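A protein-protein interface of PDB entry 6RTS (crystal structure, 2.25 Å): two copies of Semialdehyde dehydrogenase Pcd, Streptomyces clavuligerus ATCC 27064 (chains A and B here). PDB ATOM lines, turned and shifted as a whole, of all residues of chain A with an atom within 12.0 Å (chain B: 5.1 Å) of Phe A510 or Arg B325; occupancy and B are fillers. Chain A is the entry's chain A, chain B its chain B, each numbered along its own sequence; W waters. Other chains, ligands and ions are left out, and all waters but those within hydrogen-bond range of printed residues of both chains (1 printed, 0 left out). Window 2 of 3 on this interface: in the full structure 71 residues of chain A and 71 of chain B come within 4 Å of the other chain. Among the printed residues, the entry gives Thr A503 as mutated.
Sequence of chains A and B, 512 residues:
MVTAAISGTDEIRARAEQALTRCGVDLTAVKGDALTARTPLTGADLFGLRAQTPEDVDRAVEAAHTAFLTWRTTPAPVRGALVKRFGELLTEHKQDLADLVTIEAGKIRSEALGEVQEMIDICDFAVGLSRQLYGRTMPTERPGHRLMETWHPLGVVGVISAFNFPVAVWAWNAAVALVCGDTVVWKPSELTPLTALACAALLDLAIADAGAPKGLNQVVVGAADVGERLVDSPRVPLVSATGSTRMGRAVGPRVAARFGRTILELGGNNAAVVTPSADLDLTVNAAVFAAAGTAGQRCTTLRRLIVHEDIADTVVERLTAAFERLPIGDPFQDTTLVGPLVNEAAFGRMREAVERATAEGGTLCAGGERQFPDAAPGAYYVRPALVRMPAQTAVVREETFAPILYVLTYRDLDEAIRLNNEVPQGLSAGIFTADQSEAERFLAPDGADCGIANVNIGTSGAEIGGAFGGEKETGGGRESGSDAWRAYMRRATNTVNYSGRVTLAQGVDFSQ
OG of Ser A511 sits at hydrogen-bond distance from OD1 of Asp A509 (2.4 Å).
O of Leu B326 is in hydrogen-bond range of NH1 of Arg B383 (2.9 Å).
The backbone carbonyl oxygen (O) of Pro B327 lies within hydrogen-bond range of the backbone NH (N) of Leu B337.
Phe A510 touches just these residues of chain B: Asn B285 (2.7 Å), Val B288 (3.7 Å), Phe B289 (3.8 Å), Ala B322 (3.8 Å), Arg B325 (3.9 Å) and Leu B326 (3.9 Å).
Of the printed residues of chain A, Arg B325 touches Phe A510 (3.9 Å).
No residue of chain A comes within 4 Å of Val B284.
Printed residues of chain A within 4 Å of Asn B285: Val A502, Leu A504, Asp A509, Phe A510 and Ser A511.
No residue of chain A comes within 4 Å of Ala B321.
Glu B324 touches none of the printed residues of chain A.
Of chain A, only Phe A510 comes within 4 Å of Leu B326.
Printed residues of chain B within 4 Å of Leu A504: Asn B285 (3.7 Å) and Phe B289 (3.5 Å).
Of the printed residues of chain A, Leu B337 touches Ala A505 (3.7 Å).
Of the printed residues of chain A, Phe B289 touches Thr A503 (3.3 Å), Leu A504 (3.5 Å), Ala A505 (3.6 Å), Val A508 (3.4 Å) and Phe A510 (3.8 Å).
Of the printed residues of chain B, Thr A503 touches Phe B289 (3.3 Å).
Phe B323 touches none of the printed residues of chain A.
Gln A506 touches none of the printed residues of chain B.
Of the 13 printed residues of chain B, 7 touch a printed residue of chain A.
Along chain B the printed residues that touch a printed residue of chain A span positions 285 to 337.
Printed residues of chain A that touch a printed residue of chain B: Val A502, Thr A503, Leu A504, Ala A505, Val A508, Asp A509, Phe A510 and Ser A511.
The side-chain carboxylate (OD1) of Asp A509 sits at hydrogen-bond distance from the side-chain amide nitrogen (ND2) of Asn B285.
The backbone NH (N) of Phe A510 sits at hydrogen-bond distance from the side-chain amide oxygen (OD1) of Asn B285 (2.7 Å).
Water W1 lies within hydrogen-bond range of O of Phe A510 (3.2 Å) and NH2 of Arg B325 (3.3 Å).
No position is printed for both chains.
Among the printed residues, merely in contact across the chains: Val A502 with Asn B285 (3.8 Å), Thr A503 with Phe B289 (3.3 Å), Leu A504 with Asn B285 (3.7 Å), Leu A504 with Phe B289 (3.5 Å), Ala A505 with Phe B289 (3.6 Å), Ala A505 with Leu B337 (3.7 Å), Val A508 with Phe B289 (3.4 Å), Phe A510 with Val B288 (3.7 Å), Phe A510 with Phe B289 (3.8 Å), Phe A510 with Ala B322 (3.8 Å), Phe A510 with Arg B325 (3.9 Å), Phe A510 with Leu B326 (3.9 Å) and Ser A511 with Asn B285 (3.9 Å).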
ATOM      1  N   GLY A 500     -19.235  -7.645  13.294  1.00  0.00           N
ATOM      2  CA  GLY A 500     -18.899  -8.800  14.128  1.00  0.00           C
ATOM      3  C   GLY A 500     -17.426  -9.185  14.119  1.00  0.00           C
ATOM      4  O   GLY A 500     -17.048 -10.145  14.786  1.00  0.00           O
ATOM      5  N   ARG A 501     -16.585  -8.443  13.397  1.00  0.00           N
ATOM      6  CA  ARG A 501     -15.183  -8.801  13.277  1.00  0.00           C
ATOM      7  C   ARG A 501     -14.253  -7.577  13.343  1.00  0.00           C
ATOM      8  O   ARG A 501     -14.709  -6.439  13.252  1.00  0.00           O
ATOM      9  CB  ARG A 501     -14.961  -9.707  12.037  1.00  0.00           C
ATOM     10  CG  ARG A 501     -15.072  -9.093  10.641  1.00  0.00           C
ATOM     11  CD  ARG A 501     -14.612 -10.093   9.545  1.00  0.00           C
ATOM     12  NE  ARG A 501     -13.214 -10.533   9.770  1.00  0.00           N
ATOM     13  CZ  ARG A 501     -12.104  -9.809   9.530  1.00  0.00           C
ATOM     14  NH1 ARG A 501     -10.912 -10.318   9.834  1.00  0.00           N
ATOM     15  NH2 ARG A 501     -12.154  -8.589   8.992  1.00  0.00           N
ATOM     16  N   VAL A 502     -12.962  -7.850  13.538  1.00  0.00           N
ATOM     17  CA  VAL A 502     -11.912  -6.841  13.748  1.00  0.00           C
ATOM     18  C   VAL A 502     -10.713  -7.188  12.880  1.00  0.00           C
ATOM     19  O   VAL A 502     -10.449  -8.360  12.633  1.00  0.00           O
ATOM     20  CB  VAL A 502     -11.481  -6.775  15.250  1.00  0.00           C
ATOM     21  CG1 VAL A 502     -10.889  -8.087  15.751  1.00  0.00           C
ATOM     22  CG2 VAL A 502     -10.504  -5.633  15.518  1.00  0.00           C
ATOM     23  N   THR A 503      -9.985  -6.180  12.411  1.00  0.00           N
ATOM     24  CA  THR A 503      -8.707  -6.418  11.768  1.00  0.00           C
ATOM     25  C   THR A 503      -7.832  -7.218  12.716  1.00  0.00           C
ATOM     26  O   THR A 503      -7.707  -6.874  13.864  1.00  0.00           O
ATOM     27  CB  THR A 503      -8.005  -5.102  11.380  1.00  0.00           C
ATOM     28  OG1 THR A 503      -8.746  -4.465  10.332  1.00  0.00           O
ATOM     29  CG2 THR A 503      -6.576  -5.345  10.878  1.00  0.00           C
ATOM     30  N   LEU A 504      -7.287  -8.324  12.222  1.00  0.00           N
ATOM     31  CA  LEU A 504      -6.385  -9.192  12.988  1.00  0.00           C
ATOM     32  C   LEU A 504      -4.958  -8.752  12.709  1.00  0.00           C
ATOM     33  O   LEU A 504      -4.531  -8.738  11.561  1.00  0.00           O
ATOM     34  CB  LEU A 504      -6.586 -10.647  12.578  1.00  0.00           C
ATOM     35  CG  LEU A 504      -8.033 -11.148  12.737  1.00  0.00           C
ATOM     36  CD1 LEU A 504      -8.134 -12.568  12.213  1.00  0.00           C
ATOM     37  CD2 LEU A 504      -8.508 -11.093  14.178  1.00  0.00           C
ATOM     38  N   ALA A 505      -4.257  -8.335  13.751  1.00  0.00           N
ATOM     39  CA  ALA A 505      -2.923  -7.816  13.616  1.00  0.00           C
ATOM     40  C   ALA A 505      -1.996  -8.955  13.210  1.00  0.00           C
ATOM     41  O   ALA A 505      -1.973 -10.012  13.845  1.00  0.00           O
ATOM     42  CB  ALA A 505      -2.467  -7.183  14.921  1.00  0.00           C
ATOM     43  N   GLN A 506      -1.276  -8.740  12.116  1.00  0.00           N
ATOM     44  CA  GLN A 506      -0.389  -9.748  11.535  1.00  0.00           C
ATOM     45  C   GLN A 506      -1.134 -11.041  11.150  1.00  0.00           C
ATOM     46  O   GLN A 506      -0.510 -12.084  11.007  1.00  0.00           O
ATOM     47  CB  GLN A 506       0.798 -10.053  12.478  1.00  0.00           C
ATOM     48  CG  GLN A 506       1.547  -8.840  12.998  1.00  0.00           C
ATOM     49  CD  GLN A 506       2.125  -7.959  11.899  1.00  0.00           C
ATOM     50  OE1 GLN A 506       1.535  -6.935  11.543  1.00  0.00           O
ATOM     51  NE2 GLN A 506       3.279  -8.343  11.362  1.00  0.00           N
ATOM     52  N   GLY A 507      -2.457 -10.951  10.960  1.00  0.00           N
ATOM     53  CA  GLY A 507      -3.315 -12.088  10.672  1.00  0.00           C
ATOM     54  C   GLY A 507      -3.627 -13.034  11.822  1.00  0.00           C
ATOM     55  O   GLY A 507      -4.348 -14.006  11.636  1.00  0.00           O
ATOM     56  N   VAL A 508      -3.131 -12.742  13.018  1.00  0.00           N
ATOM     57  CA  VAL A 508      -3.239 -13.676  14.126  1.00  0.00           C
ATOM     58  C   VAL A 508      -4.654 -13.607  14.725  1.00  0.00           C
ATOM     59  O   VAL A 508      -5.180 -12.516  14.953  1.00  0.00           O
ATOM     60  CB  VAL A 508      -2.174 -13.388  15.200  1.00  0.00           C
ATOM     61  CG1 VAL A 508      -2.344 -14.310  16.397  1.00  0.00           C
ATOM     62  CG2 VAL A 508      -0.771 -13.538  14.610  1.00  0.00           C
ATOM     63  N   ASP A 509      -5.260 -14.775  14.950  1.00  0.00           N
ATOM     64  CA  ASP A 509      -6.566 -14.884  15.576  1.00  0.00           C
ATOM     65  C   ASP A 509      -6.378 -15.529  16.929  1.00  0.00           C
ATOM     66  O   ASP A 509      -5.991 -16.683  16.998  1.00  0.00           O
ATOM     67  CB  ASP A 509      -7.484 -15.751  14.709  1.00  0.00           C
ATOM     68  CG  ASP A 509      -8.911 -15.779  15.204  1.00  0.00           C
ATOM     69  OD1 ASP A 509      -9.192 -15.289  16.329  1.00  0.00           O
ATOM     70  OD2 ASP A 509      -9.765 -16.314  14.460  1.00  0.00           O
ATOM     71  N   PHE A 510      -6.659 -14.802  18.009  1.00  0.00           N
ATOM     72  CA  PHE A 510      -6.502 -15.355  19.367  1.00  0.00           C
ATOM     73  C   PHE A 510      -7.705 -16.163  19.888  1.00  0.00           C
ATOM     74  O   PHE A 510      -7.687 -16.582  21.038  1.00  0.00           O
ATOM     75  CB  PHE A 510      -6.080 -14.267  20.362  1.00  0.00           C
ATOM     76  CG  PHE A 510      -4.654 -13.830  20.189  1.00  0.00           C
ATOM     77  CD1 PHE A 510      -3.610 -14.634  20.650  1.00  0.00           C
ATOM     78  CD2 PHE A 510      -4.339 -12.636  19.559  1.00  0.00           C
ATOM     79  CE1 PHE A 510      -2.283 -14.254  20.481  1.00  0.00           C
ATOM     80  CE2 PHE A 510      -3.011 -12.259  19.378  1.00  0.00           C
ATOM     81  CZ  PHE A 510      -1.979 -13.068  19.843  1.00  0.00           C
ATOM     82  N   SER A 511      -8.708 -16.433  19.046  1.00  0.00           N
ATOM     83  CA  SER A 511      -9.886 -17.227  19.464  1.00  0.00           C
ATOM     84  C   SER A 511      -9.819 -18.728  19.114  1.00  0.00           C
ATOM     85  O   SER A 511      -8.742 -19.302  18.940  1.00  0.00           O
ATOM     86  CB  SER A 511     -11.158 -16.618  18.868  1.00  0.00           C
ATOM     87  OG  SER A 511     -11.046 -16.346  17.480  1.00  0.00           O
ATOM     88  N   VAL B 284     -11.701 -10.344  22.742  1.00  0.00           N
ATOM     89  CA  VAL B 284     -10.333 -10.771  23.039  1.00  0.00           C
ATOM     90  C   VAL B 284      -9.333 -10.351  21.965  1.00  0.00           C
ATOM     91  O   VAL B 284      -8.263  -9.836  22.287  1.00  0.00           O
ATOM     92  CB  VAL B 284     -10.248 -12.295  23.330  1.00  0.00           C
ATOM     93  CG1 VAL B 284      -8.797 -12.760  23.448  1.00  0.00           C
ATOM     94  CG2 VAL B 284     -11.006 -12.630  24.615  1.00  0.00           C
ATOM     95  N   ASN B 285      -9.677 -10.536  20.693  1.00  0.00           N
ATOM     96  CA  ASN B 285      -8.810 -10.040  19.618  1.00  0.00           C
ATOM     97  C   ASN B 285      -8.669  -8.522  19.670  1.00  0.00           C
ATOM     98  O   ASN B 285      -7.575  -8.004  19.580  1.00  0.00           O
ATOM     99  CB  ASN B 285      -9.310 -10.489  18.237  1.00  0.00           C
ATOM    100  CG  ASN B 285      -9.030 -11.972  17.960  1.00  0.00           C
ATOM    101  OD1 ASN B 285      -7.985 -12.487  18.365  1.00  0.00           O
ATOM    102  ND2 ASN B 285      -9.949 -12.659  17.243  1.00  0.00           N
ATOM    103  N   VAL B 288      -6.565  -7.365  22.866  1.00  0.00           N
ATOM    104  CA  VAL B 288      -5.143  -7.716  22.722  1.00  0.00           C
ATOM    105  C   VAL B 288      -4.415  -6.778  21.786  1.00  0.00           C
ATOM    106  O   VAL B 288      -3.309  -6.323  22.068  1.00  0.00           O
ATOM    107  CB  VAL B 288      -4.952  -9.186  22.233  1.00  0.00           C
ATOM    108  CG1 VAL B 288      -3.525  -9.464  21.754  1.00  0.00           C
ATOM    109  CG2 VAL B 288      -5.319 -10.162  23.328  1.00  0.00           C
ATOM    110  N   PHE B 289      -5.016  -6.497  20.657  1.00  0.00           N
ATOM    111  CA  PHE B 289      -4.359  -5.670  19.657  1.00  0.00           C
ATOM    112  C   PHE B 289      -4.226  -4.232  20.134  1.00  0.00           C
ATOM    113  O   PHE B 289      -3.189  -3.597  19.923  1.00  0.00           O
ATOM    114  CB  PHE B 289      -5.123  -5.700  18.339  1.00  0.00           C
ATOM    115  CG  PHE B 289      -5.342  -7.101  17.764  1.00  0.00           C
ATOM    116  CD1 PHE B 289      -4.423  -8.148  17.964  1.00  0.00           C
ATOM    117  CD2 PHE B 289      -6.479  -7.360  16.984  1.00  0.00           C
ATOM    118  CE1 PHE B 289      -4.661  -9.415  17.420  1.00  0.00           C
ATOM    119  CE2 PHE B 289      -6.713  -8.630  16.460  1.00  0.00           C
ATOM    120  CZ  PHE B 289      -5.810  -9.654  16.675  1.00  0.00           C
ATOM    121  N   ALA B 321      -4.103 -16.321  28.472  1.00  0.00           N
ATOM    122  CA  ALA B 321      -3.582 -17.230  27.456  1.00  0.00           C
ATOM    123  C   ALA B 321      -3.056 -16.477  26.217  1.00  0.00           C
ATOM    124  O   ALA B 321      -1.995 -16.825  25.681  1.00  0.00           O
ATOM    125  CB  ALA B 321      -4.648 -18.245  27.053  1.00  0.00           C
ATOM    126  N   ALA B 322      -3.784 -15.438  25.781  1.00  0.00           N
ATOM    127  CA  ALA B 322      -3.367 -14.652  24.622  1.00  0.00           C
ATOM    128  C   ALA B 322      -2.079 -13.891  24.916  1.00  0.00           C
ATOM    129  O   ALA B 322      -1.162 -13.901  24.090  1.00  0.00           O
ATOM    130  CB  ALA B 322      -4.472 -13.693  24.190  1.00  0.00           C
ATOM    131  N   PHE B 323      -2.010 -13.229  26.081  1.00  0.00           N
ATOM    132  CA  PHE B 323      -0.800 -12.478  26.463  1.00  0.00           C
ATOM    133  C   PHE B 323       0.448 -13.376  26.541  1.00  0.00           C
ATOM    134  O   PHE B 323       1.532 -12.953  26.157  1.00  0.00           O
ATOM    135  CB  PHE B 323      -0.983 -11.740  27.795  1.00  0.00           C
ATOM    136  CG  PHE B 323      -1.575 -10.349  27.667  1.00  0.00           C
ATOM    137  CD1 PHE B 323      -2.738 -10.118  26.922  1.00  0.00           C
ATOM    138  CD2 PHE B 323      -0.999  -9.274  28.341  1.00  0.00           C
ATOM    139  CE1 PHE B 323      -3.290  -8.831  26.846  1.00  0.00           C
ATOM    140  CE2 PHE B 323      -1.539  -8.003  28.259  1.00  0.00           C
ATOM    141  CZ  PHE B 323      -2.688  -7.781  27.527  1.00  0.00           C
ATOM    142  N   GLU B 324       0.277 -14.603  27.033  1.00  0.00           N
ATOM    143  CA  GLU B 324       1.364 -15.582  27.102  1.00  0.00           C
ATOM    144  C   GLU B 324       1.881 -16.044  25.743  1.00  0.00           C
ATOM    145  O   GLU B 324       3.046 -16.393  25.646  1.00  0.00           O
ATOM    146  CB  GLU B 324       0.923 -16.801  27.905  1.00  0.00           C
ATOM    147  CG  GLU B 324       0.856 -16.533  29.399  1.00  0.00           C
ATOM    148  CD  GLU B 324       0.124 -17.616  30.157  1.00  0.00           C
ATOM    149  OE1 GLU B 324      -0.587 -18.438  29.532  1.00  0.00           O
ATOM    150  OE2 GLU B 324       0.240 -17.630  31.400  1.00  0.00           O
ATOM    151  N   ARG B 325       1.009 -16.047  24.730  1.00  0.00           N
ATOM    152  CA  ARG B 325       1.322 -16.381  23.340  1.00  0.00           C
ATOM    153  C   ARG B 325       1.839 -15.219  22.466  1.00  0.00           C
ATOM    154  O   ARG B 325       2.277 -15.466  21.355  1.00  0.00           O
ATOM    155  CB  ARG B 325       0.062 -16.906  22.638  1.00  0.00           C
ATOM    156  CG  ARG B 325      -0.447 -18.310  23.019  1.00  0.00           C
ATOM    157  CD  ARG B 325      -1.656 -18.691  22.144  1.00  0.00           C
ATOM    158  NE  ARG B 325      -1.387 -18.476  20.698  1.00  0.00           N
ATOM    159  CZ  ARG B 325      -2.305 -18.359  19.724  1.00  0.00           C
ATOM    160  NH1 ARG B 325      -1.898 -18.145  18.463  1.00  0.00           N
ATOM    161  NH2 ARG B 325      -3.613 -18.451  19.991  1.00  0.00           N
ATOM    162  N   LEU B 326       1.761 -13.969  22.913  1.00  0.00           N
ATOM    163  CA  LEU B 326       2.194 -12.841  22.078  1.00  0.00           C
ATOM    164  C   LEU B 326       3.661 -12.982  21.649  1.00  0.00           C
ATOM    165  O   LEU B 326       4.528 -13.146  22.509  1.00  0.00           O
ATOM    166  CB  LEU B 326       2.049 -11.500  22.819  1.00  0.00           C
ATOM    167  CG  LEU B 326       0.659 -10.927  23.033  1.00  0.00           C
ATOM    168  CD1 LEU B 326       0.733  -9.796  24.036  1.00  0.00           C
ATOM    169  CD2 LEU B 326       0.084 -10.415  21.732  1.00  0.00           C
ATOM    170  N   PRO B 327       3.938 -12.910  20.329  1.00  0.00           N
ATOM    171  CA  PRO B 327       5.328 -12.937  19.862  1.00  0.00           C
ATOM    172  C   PRO B 327       5.985 -11.598  19.972  1.00  0.00           C
ATOM    173  O   PRO B 327       5.514 -10.630  19.389  1.00  0.00           O
ATOM    174  CB  PRO B 327       5.221 -13.354  18.390  1.00  0.00           C
ATOM    175  CG  PRO B 327       3.828 -13.020  17.985  1.00  0.00           C
ATOM    176  CD  PRO B 327       2.967 -12.993  19.215  1.00  0.00           C
ATOM    177  N   LEU B 337       4.856  -9.270  16.753  1.00  0.00           N
ATOM    178  CA  LEU B 337       3.690  -8.436  17.043  1.00  0.00           C
ATOM    179  C   LEU B 337       4.013  -7.273  18.002  1.00  0.00           C
ATOM    180  O   LEU B 337       3.475  -6.183  17.849  1.00  0.00           O
ATOM    181  CB  LEU B 337       2.559  -9.301  17.592  1.00  0.00           C
ATOM    182  CG  LEU B 337       1.266  -8.574  17.997  1.00  0.00           C
ATOM    183  CD1 LEU B 337       0.696  -7.735  16.852  1.00  0.00           C
ATOM    184  CD2 LEU B 337       0.231  -9.584  18.471  1.00  0.00           C
ATOM    185  N   ARG B 383       7.078  -8.318  27.669  1.00  0.00           N
ATOM    186  CA  ARG B 383       5.773  -8.894  27.420  1.00  0.00           C
ATOM    187  C   ARG B 383       4.751  -7.994  28.099  1.00  0.00           C
ATOM    188  O   ARG B 383       4.897  -7.662  29.294  1.00  0.00           O
ATOM    189  CB  ARG B 383       5.696 -10.315  27.966  1.00  0.00           C
ATOM    190  CG  ARG B 383       4.368 -11.027  27.726  1.00  0.00           C
ATOM    191  CD  ARG B 383       4.438 -12.513  28.134  1.00  0.00           C
ATOM    192  NE  ARG B 383       5.472 -13.230  27.384  1.00  0.00           N
ATOM    193  CZ  ARG B 383       5.365 -13.612  26.109  1.00  0.00           C
ATOM    194  NH1 ARG B 383       4.263 -13.383  25.375  1.00  0.00           N
ATOM    195  NH2 ARG B 383       6.387 -14.234  25.553  1.00  0.00           N
HETATM  196  O   HOH W   1      -5.082 -17.500  22.748  1.00  0.00           O
